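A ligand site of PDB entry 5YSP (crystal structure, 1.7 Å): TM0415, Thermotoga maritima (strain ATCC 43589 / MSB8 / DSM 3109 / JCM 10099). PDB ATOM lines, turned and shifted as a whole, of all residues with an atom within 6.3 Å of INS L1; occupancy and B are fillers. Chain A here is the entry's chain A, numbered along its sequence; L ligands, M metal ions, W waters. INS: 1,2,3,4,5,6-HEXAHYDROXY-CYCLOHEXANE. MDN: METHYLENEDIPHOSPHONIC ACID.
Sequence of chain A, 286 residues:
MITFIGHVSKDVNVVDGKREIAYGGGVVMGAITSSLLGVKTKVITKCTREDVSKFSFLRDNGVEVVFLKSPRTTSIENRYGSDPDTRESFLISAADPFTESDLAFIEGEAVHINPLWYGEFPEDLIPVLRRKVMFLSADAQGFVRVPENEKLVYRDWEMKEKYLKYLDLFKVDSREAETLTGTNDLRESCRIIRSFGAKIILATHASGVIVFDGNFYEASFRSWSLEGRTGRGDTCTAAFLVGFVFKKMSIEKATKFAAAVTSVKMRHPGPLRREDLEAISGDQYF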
ATOM      1  N   SER A   9      15.100  -9.238  26.799  1.00  0.00           N
ATOM      2  CA  SER A   9      16.282  -8.576  26.264  1.00  0.00           C
ATOM      3  C   SER A   9      16.389  -8.697  24.775  1.00  0.00           C
ATOM      4  O   SER A   9      16.105  -9.757  24.240  1.00  0.00           O
ATOM      5  CB  SER A   9      17.541  -9.164  26.888  1.00  0.00           C
ATOM      6  OG  SER A   9      18.732  -8.596  26.363  1.00  0.00           O
ATOM      7  N   LYS A  10      16.771  -7.610  24.144  1.00  0.00           N
ATOM      8  CA  LYS A  10      17.303  -7.654  22.788  1.00  0.00           C
ATOM      9  C   LYS A  10      18.779  -8.052  22.942  1.00  0.00           C
ATOM     10  O   LYS A  10      19.634  -7.218  23.298  1.00  0.00           O
ATOM     11  CB  LYS A  10      17.163  -6.300  22.085  1.00  0.00           C
ATOM     12  CG  LYS A  10      17.834  -6.242  20.714  1.00  0.00           C
ATOM     13  CD  LYS A  10      17.910  -4.833  20.165  1.00  0.00           C
ATOM     14  CE  LYS A  10      18.375  -4.900  18.736  1.00  0.00           C
ATOM     15  NZ  LYS A  10      18.440  -3.568  18.109  1.00  0.00           N
ATOM     16  N   ASP A  11      19.069  -9.307  22.648  1.00  0.00           N
ATOM     17  CA  ASP A  11      20.447  -9.790  22.721  1.00  0.00           C
ATOM     18  C   ASP A  11      21.179  -9.463  21.418  1.00  0.00           C
ATOM     19  O   ASP A  11      20.678  -9.780  20.327  1.00  0.00           O
ATOM     20  CB  ASP A  11      20.477 -11.296  22.944  1.00  0.00           C
ATOM     21  CG  ASP A  11      19.963 -11.688  24.348  1.00  0.00           C
ATOM     22  OD1 ASP A  11      19.889 -10.837  25.253  1.00  0.00           O
ATOM     23  OD2 ASP A  11      19.687 -12.879  24.542  1.00  0.00           O
ATOM     24  N   VAL A  12      22.363  -8.873  21.556  1.00  0.00           N
ATOM     25  CA  VAL A  12      23.252  -8.604  20.419  1.00  0.00           C
ATOM     26  C   VAL A  12      24.403  -9.591  20.539  1.00  0.00           C
ATOM     27  O   VAL A  12      25.289  -9.382  21.347  1.00  0.00           O
ATOM     28  CB  VAL A  12      23.764  -7.155  20.420  1.00  0.00           C
ATOM     29  CG1 VAL A  12      24.673  -6.898  19.212  1.00  0.00           C
ATOM     30  CG2 VAL A  12      22.590  -6.176  20.470  1.00  0.00           C
ATOM     31  N   ASN A  13      24.349 -10.663  19.763  1.00  0.00           N
ATOM     32  CA  ASN A  13      25.307 -11.737  19.871  1.00  0.00           C
ATOM     33  C   ASN A  13      26.364 -11.549  18.798  1.00  0.00           C
ATOM     34  O   ASN A  13      26.043 -11.431  17.618  1.00  0.00           O
ATOM     35  CB  ASN A  13      24.617 -13.090  19.760  1.00  0.00           C
ATOM     36  CG  ASN A  13      23.649 -13.315  20.887  1.00  0.00           C
ATOM     37  OD1 ASN A  13      23.929 -12.951  22.050  1.00  0.00           O
ATOM     38  ND2 ASN A  13      22.471 -13.856  20.578  1.00  0.00           N
ATOM     39  N   GLY A  24      15.259 -12.444  23.563  1.00  0.00           N
ATOM     40  CA  GLY A  24      15.244 -13.482  24.583  1.00  0.00           C
ATOM     41  C   GLY A  24      15.194 -12.891  25.989  1.00  0.00           C
ATOM     42  O   GLY A  24      14.368 -11.980  26.258  1.00  0.00           O
ATOM     43  N   GLY A  25      16.076 -13.437  26.833  1.00  0.00           N
ATOM     44  CA  GLY A  25      16.136 -13.139  28.272  1.00  0.00           C
ATOM     45  C   GLY A  25      15.901 -14.376  29.105  1.00  0.00           C
ATOM     46  O   GLY A  25      15.375 -15.399  28.626  1.00  0.00           O
ATOM     47  N   GLY A  26      16.272 -14.292  30.373  1.00  0.00           N
ATOM     48  CA  GLY A  26      16.104 -15.418  31.274  1.00  0.00           C
ATOM     49  C   GLY A  26      14.646 -15.857  31.374  1.00  0.00           C
ATOM     50  O   GLY A  26      14.340 -17.070  31.337  1.00  0.00           O
ATOM     51  N   MET A  29      13.436 -17.924  28.297  1.00  0.00           N
ATOM     52  CA  MET A  29      13.925 -19.285  28.352  1.00  0.00           C
ATOM     53  C   MET A  29      13.184 -20.131  29.403  1.00  0.00           C
ATOM     54  O   MET A  29      12.761 -21.228  29.114  1.00  0.00           O
ATOM     55  CB  MET A  29      15.423 -19.309  28.613  1.00  0.00           C
ATOM     56  CG  MET A  29      16.246 -18.727  27.474  1.00  0.00           C
ATOM     57  SD  MET A  29      16.328 -19.915  26.121  1.00  0.00           S
ATOM     58  CE  MET A  29      17.388 -19.019  24.978  1.00  0.00           C
ATOM     59  N   ILE A  76      21.497  -6.515  25.793  1.00  0.00           N
ATOM     60  CA  ILE A  76      22.762  -7.009  26.244  1.00  0.00           C
ATOM     61  C   ILE A  76      23.538  -7.498  25.013  1.00  0.00           C
ATOM     62  O   ILE A  76      23.019  -8.292  24.206  1.00  0.00           O
ATOM     63  CB  ILE A  76      22.583  -8.146  27.260  1.00  0.00           C
ATOM     64  CG1 ILE A  76      21.984  -7.573  28.540  1.00  0.00           C
ATOM     65  CG2 ILE A  76      23.903  -8.858  27.564  1.00  0.00           C
ATOM     66  CD1 ILE A  76      21.362  -8.588  29.452  1.00  0.00           C
ATOM     67  N   GLU A  77      24.783  -7.045  24.930  1.00  0.00           N
ATOM     68  CA  GLU A  77      25.730  -7.614  23.941  1.00  0.00           C
ATOM     69  C   GLU A  77      26.528  -8.755  24.555  1.00  0.00           C
ATOM     70  O   GLU A  77      27.115  -8.604  25.642  1.00  0.00           O
ATOM     71  CB  GLU A  77      26.658  -6.542  23.397  1.00  0.00           C
ATOM     72  CG  GLU A  77      27.615  -7.088  22.339  1.00  0.00           C
ATOM     73  CD  GLU A  77      28.564  -6.051  21.813  1.00  0.00           C
ATOM     74  OE1 GLU A  77      28.115  -4.986  21.408  1.00  0.00           O
ATOM     75  OE2 GLU A  77      29.768  -6.318  21.824  1.00  0.00           O
ATOM     76  N   ASN A  78      26.548  -9.911  23.873  1.00  0.00           N
ATOM     77  CA  ASN A  78      27.307 -11.059  24.298  1.00  0.00           C
ATOM     78  C   ASN A  78      28.385 -11.320  23.277  1.00  0.00           C
ATOM     79  O   ASN A  78      28.075 -11.528  22.109  1.00  0.00           O
ATOM     80  CB  ASN A  78      26.409 -12.285  24.376  1.00  0.00           C
ATOM     81  CG  ASN A  78      25.274 -12.086  25.335  1.00  0.00           C
ATOM     82  OD1 ASN A  78      25.511 -11.762  26.505  1.00  0.00           O
ATOM     83  ND2 ASN A  78      24.044 -12.212  24.843  1.00  0.00           N
ATOM     84  N   TYR A  80      31.457 -13.956  22.416  1.00  0.00           N
ATOM     85  CA  TYR A  80      31.791 -15.350  22.779  1.00  0.00           C
ATOM     86  C   TYR A  80      33.239 -15.714  22.465  1.00  0.00           C
ATOM     87  O   TYR A  80      34.045 -14.855  22.141  1.00  0.00           O
ATOM     88  CB  TYR A  80      30.843 -16.319  22.078  1.00  0.00           C
ATOM     89  CG  TYR A  80      29.459 -16.255  22.627  1.00  0.00           C
ATOM     90  CD1 TYR A  80      28.515 -15.389  22.069  1.00  0.00           C
ATOM     91  CD2 TYR A  80      29.070 -17.053  23.721  1.00  0.00           C
ATOM     92  CE1 TYR A  80      27.223 -15.318  22.574  1.00  0.00           C
ATOM     93  CE2 TYR A  80      27.793 -16.990  24.237  1.00  0.00           C
ATOM     94  CZ  TYR A  80      26.871 -16.120  23.671  1.00  0.00           C
ATOM     95  OH  TYR A  80      25.609 -16.049  24.173  1.00  0.00           O
ATOM     96  N   SER A  89      29.823 -10.030  28.526  1.00  0.00           N
ATOM     97  CA  SER A  89      28.582  -9.345  28.207  1.00  0.00           C
ATOM     98  C   SER A  89      28.589  -7.872  28.620  1.00  0.00           C
ATOM     99  O   SER A  89      29.298  -7.461  29.523  1.00  0.00           O
ATOM    100  CB  SER A  89      27.373 -10.079  28.814  1.00  0.00           C
ATOM    101  OG  SER A  89      27.414 -11.438  28.442  1.00  0.00           O
ATOM    102  N   PRO A 115      16.623 -12.097  37.051  1.00  0.00           N
ATOM    103  CA  PRO A 115      17.104 -10.835  36.494  1.00  0.00           C
ATOM    104  C   PRO A 115      18.362 -10.985  35.684  1.00  0.00           C
ATOM    105  O   PRO A 115      19.081 -11.968  35.849  1.00  0.00           O
ATOM    106  CB  PRO A 115      17.356  -9.960  37.734  1.00  0.00           C
ATOM    107  CG  PRO A 115      16.976 -10.848  38.914  1.00  0.00           C
ATOM    108  CD  PRO A 115      17.080 -12.252  38.443  1.00  0.00           C
ATOM    109  N   LEU A 116      18.591 -10.020  34.799  1.00  0.00           N
ATOM    110  CA  LEU A 116      19.766 -10.026  33.934  1.00  0.00           C
ATOM    111  C   LEU A 116      20.960  -9.213  34.464  1.00  0.00           C
ATOM    112  O   LEU A 116      22.107  -9.409  33.984  1.00  0.00           O
ATOM    113  CB  LEU A 116      19.362  -9.489  32.560  1.00  0.00           C
ATOM    114  CG  LEU A 116      18.312 -10.305  31.801  1.00  0.00           C
ATOM    115  CD1 LEU A 116      17.881  -9.546  30.558  1.00  0.00           C
ATOM    116  CD2 LEU A 116      18.808 -11.704  31.491  1.00  0.00           C
ATOM    117  N   GLN A 141      22.614 -14.603  38.751  1.00  0.00           N
ATOM    118  CA  GLN A 141      22.956 -13.605  37.724  1.00  0.00           C
ATOM    119  C   GLN A 141      22.434 -12.216  38.115  1.00  0.00           C
ATOM    120  O   GLN A 141      23.127 -11.209  37.961  1.00  0.00           O
ATOM    121  CB  GLN A 141      22.381 -14.002  36.398  1.00  0.00           C
ATOM    122  CG  GLN A 141      22.692 -12.980  35.322  1.00  0.00           C
ATOM    123  CD  GLN A 141      22.300 -13.479  33.986  1.00  0.00           C
ATOM    124  OE1 GLN A 141      23.146 -13.998  33.278  1.00  0.00           O
ATOM    125  NE2 GLN A 141      21.035 -13.390  33.667  1.00  0.00           N
ATOM    126  N   ARG A 145      26.012 -10.016  38.675  1.00  0.00           N
ATOM    127  CA  ARG A 145      26.430  -9.451  37.402  1.00  0.00           C
ATOM    128  C   ARG A 145      26.083  -7.956  37.333  1.00  0.00           C
ATOM    129  O   ARG A 145      24.902  -7.581  37.247  1.00  0.00           O
ATOM    130  CB  ARG A 145      25.842 -10.269  36.249  1.00  0.00           C
ATOM    131  CG  ARG A 145      26.424  -9.875  34.957  1.00  0.00           C
ATOM    132  CD  ARG A 145      26.081 -10.858  33.867  1.00  0.00           C
ATOM    133  NE  ARG A 145      24.698 -10.701  33.409  1.00  0.00           N
ATOM    134  CZ  ARG A 145      24.246 -11.138  32.237  1.00  0.00           C
ATOM    135  NH1 ARG A 145      25.066 -11.777  31.381  1.00  0.00           N
ATOM    136  NH2 ARG A 145      22.988 -10.925  31.893  1.00  0.00           N
ATOM    137  N   LEU A 152      29.454  -5.999  32.025  1.00  0.00           N
ATOM    138  CA  LEU A 152      28.817  -6.740  33.109  1.00  0.00           C
ATOM    139  C   LEU A 152      29.923  -7.530  33.818  1.00  0.00           C
ATOM    140  O   LEU A 152      30.465  -8.524  33.298  1.00  0.00           O
ATOM    141  CB  LEU A 152      27.681  -7.617  32.563  1.00  0.00           C
ATOM    142  CG  LEU A 152      26.382  -6.876  32.199  1.00  0.00           C
ATOM    143  CD1 LEU A 152      25.450  -7.699  31.315  1.00  0.00           C
ATOM    144  CD2 LEU A 152      25.610  -6.423  33.433  1.00  0.00           C
ATOM    145  N   THR A 230      23.246 -20.744  25.404  1.00  0.00           N
ATOM    146  CA  THR A 230      22.541 -19.602  26.033  1.00  0.00           C
ATOM    147  C   THR A 230      21.138 -20.038  26.446  1.00  0.00           C
ATOM    148  O   THR A 230      20.422 -20.674  25.673  1.00  0.00           O
ATOM    149  CB  THR A 230      22.428 -18.372  25.109  1.00  0.00           C
ATOM    150  OG1 THR A 230      23.731 -17.892  24.770  1.00  0.00           O
ATOM    151  CG2 THR A 230      21.696 -17.252  25.830  1.00  0.00           C
ATOM    152  N   GLY A 231      20.787 -19.766  27.699  1.00  0.00           N
ATOM    153  CA  GLY A 231      19.554 -20.282  28.264  1.00  0.00           C
ATOM    154  C   GLY A 231      19.534 -21.699  28.805  1.00  0.00           C
ATOM    155  O   GLY A 231      18.485 -22.154  29.265  1.00  0.00           O
ATOM    156  N   ASP A 234      18.627 -21.287  32.592  1.00  0.00           N
ATOM    157  CA  ASP A 234      17.210 -20.900  32.754  1.00  0.00           C
ATOM    158  C   ASP A 234      16.270 -22.014  32.425  1.00  0.00           C
ATOM    159  O   ASP A 234      15.288 -22.248  33.145  1.00  0.00           O
ATOM    160  CB  ASP A 234      16.930 -19.636  31.966  1.00  0.00           C
ATOM    161  CG  ASP A 234      17.644 -18.453  32.573  1.00  0.00           C
ATOM    162  OD1 ASP A 234      17.643 -18.305  33.815  1.00  0.00           O
ATOM    163  OD2 ASP A 234      18.299 -17.719  31.861  1.00  0.00           O
HETATM  164  C1  INS L   1      21.516 -15.170  29.207  1.00  0.00           C
HETATM  165  C2  INS L   1      22.597 -14.172  29.608  1.00  0.00           C
HETATM  166  C3  INS L   1      22.907 -13.268  28.426  1.00  0.00           C
HETATM  167  C4  INS L   1      21.640 -12.522  27.986  1.00  0.00           C
HETATM  168  C5  INS L   1      20.514 -13.504  27.638  1.00  0.00           C
HETATM  169  C6  INS L   1      20.217 -14.507  28.748  1.00  0.00           C
HETATM  170  O1  INS L   1      21.212 -16.035  30.305  1.00  0.00           O
HETATM  171  O2  INS L   1      22.221 -13.378  30.742  1.00  0.00           O
HETATM  172  O3  INS L   1      23.937 -12.332  28.756  1.00  0.00           O
HETATM  173  O4  INS L   1      21.940 -11.685  26.874  1.00  0.00           O
HETATM  174  O5  INS L   1      19.308 -12.765  27.404  1.00  0.00           O
HETATM  175  O6  INS L   1      19.249 -15.462  28.304  1.00  0.00           O
HETATM  176  O3  MDN L   2      22.211 -18.481  29.721  1.00  0.00           O
HETATM  177  P1  MDN L   2      22.192 -19.127  31.189  1.00  0.00           P
HETATM  178  O1  MDN L   2      20.938 -19.886  31.417  1.00  0.00           O
HETATM  179  O2  MDN L   2      22.342 -17.977  32.316  1.00  0.00           O
HETATM  180  C4  MDN L   2      23.618 -20.259  31.182  1.00  0.00           C
HETATM  181  P5  MDN L   2      24.062 -20.989  32.793  1.00  0.00           P
HETATM  182  O6  MDN L   2      23.874 -22.460  32.768  1.00  0.00           O
HETATM  183  O7  MDN L   2      25.644 -20.677  32.887  1.00  0.00           O
HETATM  184  O8  MDN L   2      23.326 -20.333  34.043  1.00  0.00           O
HETATM  185 MG    MG M   1      22.680 -18.412  34.254  1.00  0.00          MG
HETATM  186  O   HOH W   1      18.115 -15.120  25.617  1.00  0.00           O
HETATM  187  O   HOH W   2      19.844 -15.478  32.425  1.00  0.00           O
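The side-chain carboxylate (OD1) of Asp 11 sits at hydrogen-bond distance from an oxygen (O4) of INS L1 (2.7 Å).
The side-chain amide oxygen of Gln 141 sits at hydrogen-bond distance from an oxygen (O2) of INS L1 (2.8 Å).
O3 of INS L1 lies within hydrogen-bond range of OD1 of Asn 78, 2.8 Å away.
The guanidinium group (NH2) of Arg 145 sits at hydrogen-bond distance from an oxygen (O2) of INS L1, 2.8 Å away.
The backbone NH (N) of Gly 25 lies close to an oxygen (O5) of INS L1, 3.4 Å away.
The backbone NH of Asp 234 is in hydrogen-bond range of an oxygen (O1) of MDN L2 (2.9 Å).
An oxygen (O3) of MDN L2 is in hydrogen-bond range of the backbone NH (N) of Gly 231 (2.8 Å).
An oxygen (O1) of INS L1 sits at hydrogen-bond distance from an oxygen (O3) of MDN L2.
OG of Ser 9 lies within hydrogen-bond range of OD1 of Asp 11, at 2.8 Å.
The side-chain amide nitrogen (NE2) of Gln 141 lies within hydrogen-bond range of the backbone carbonyl oxygen (O) of Pro 115.
The side-chain amide oxygen (OD1) of Asn 13 sits at hydrogen-bond distance from the side-chain amide nitrogen (ND2) of Asn 78, at 2.9 Å.
O of Val 12 sits at hydrogen-bond distance from N of Asn 78, 2.9 Å away.
NH2 of Arg 145 lies within hydrogen-bond range of O of Leu 116, 2.7 Å away.
The backbone carbonyl oxygen (O) of Ile 76 sits at hydrogen-bond distance from the backbone NH (N) of Val 12 (2.8 Å).
O of Ser 89 lies within hydrogen-bond range of N of Leu 152, at 2.9 Å.
The side-chain hydroxyl of Thr 230 lies within hydrogen-bond range of the side-chain hydroxyl of Tyr 80, at 2.7 Å.
Gly 26 touches INS L1.
Ile 76 touches INS L1 (CG2 to O4, 3.5 Å).
OG of Ser 89 touches O3 of INS L1, at 3.6 Å.
Leu 116 touches INS L1 (CD2 to O2, 3.9 Å).
CG2 of Thr 230 touches O6 of INS L1, 3.9 Å away.
Asp 234 touches INS L1.
Hydrophobic or aromatic side chains within 4 Å of INS L1: Ile 76 and Leu 116.
Within 4 Å of INS L1: Asp 11, Gly 25, Gly 26, Ile 76, Asn 78, Ser 89, Leu 116, Gln 141, Arg 145, Thr 230 and Asp 234.
The nearest printed residue that does not touch INS L1 is Ser 9 (4.04 Å).
Water W2 lies within hydrogen-bond range of O1 of INS L1, NE2 of Gln 141 and OD2 of Asp 234.
Water W1 lies within hydrogen-bond range of N of Gly 25 (2.9 Å), O6 of INS L1 (2.9 Å) and OD2 of Asp 11 (2.9 Å).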
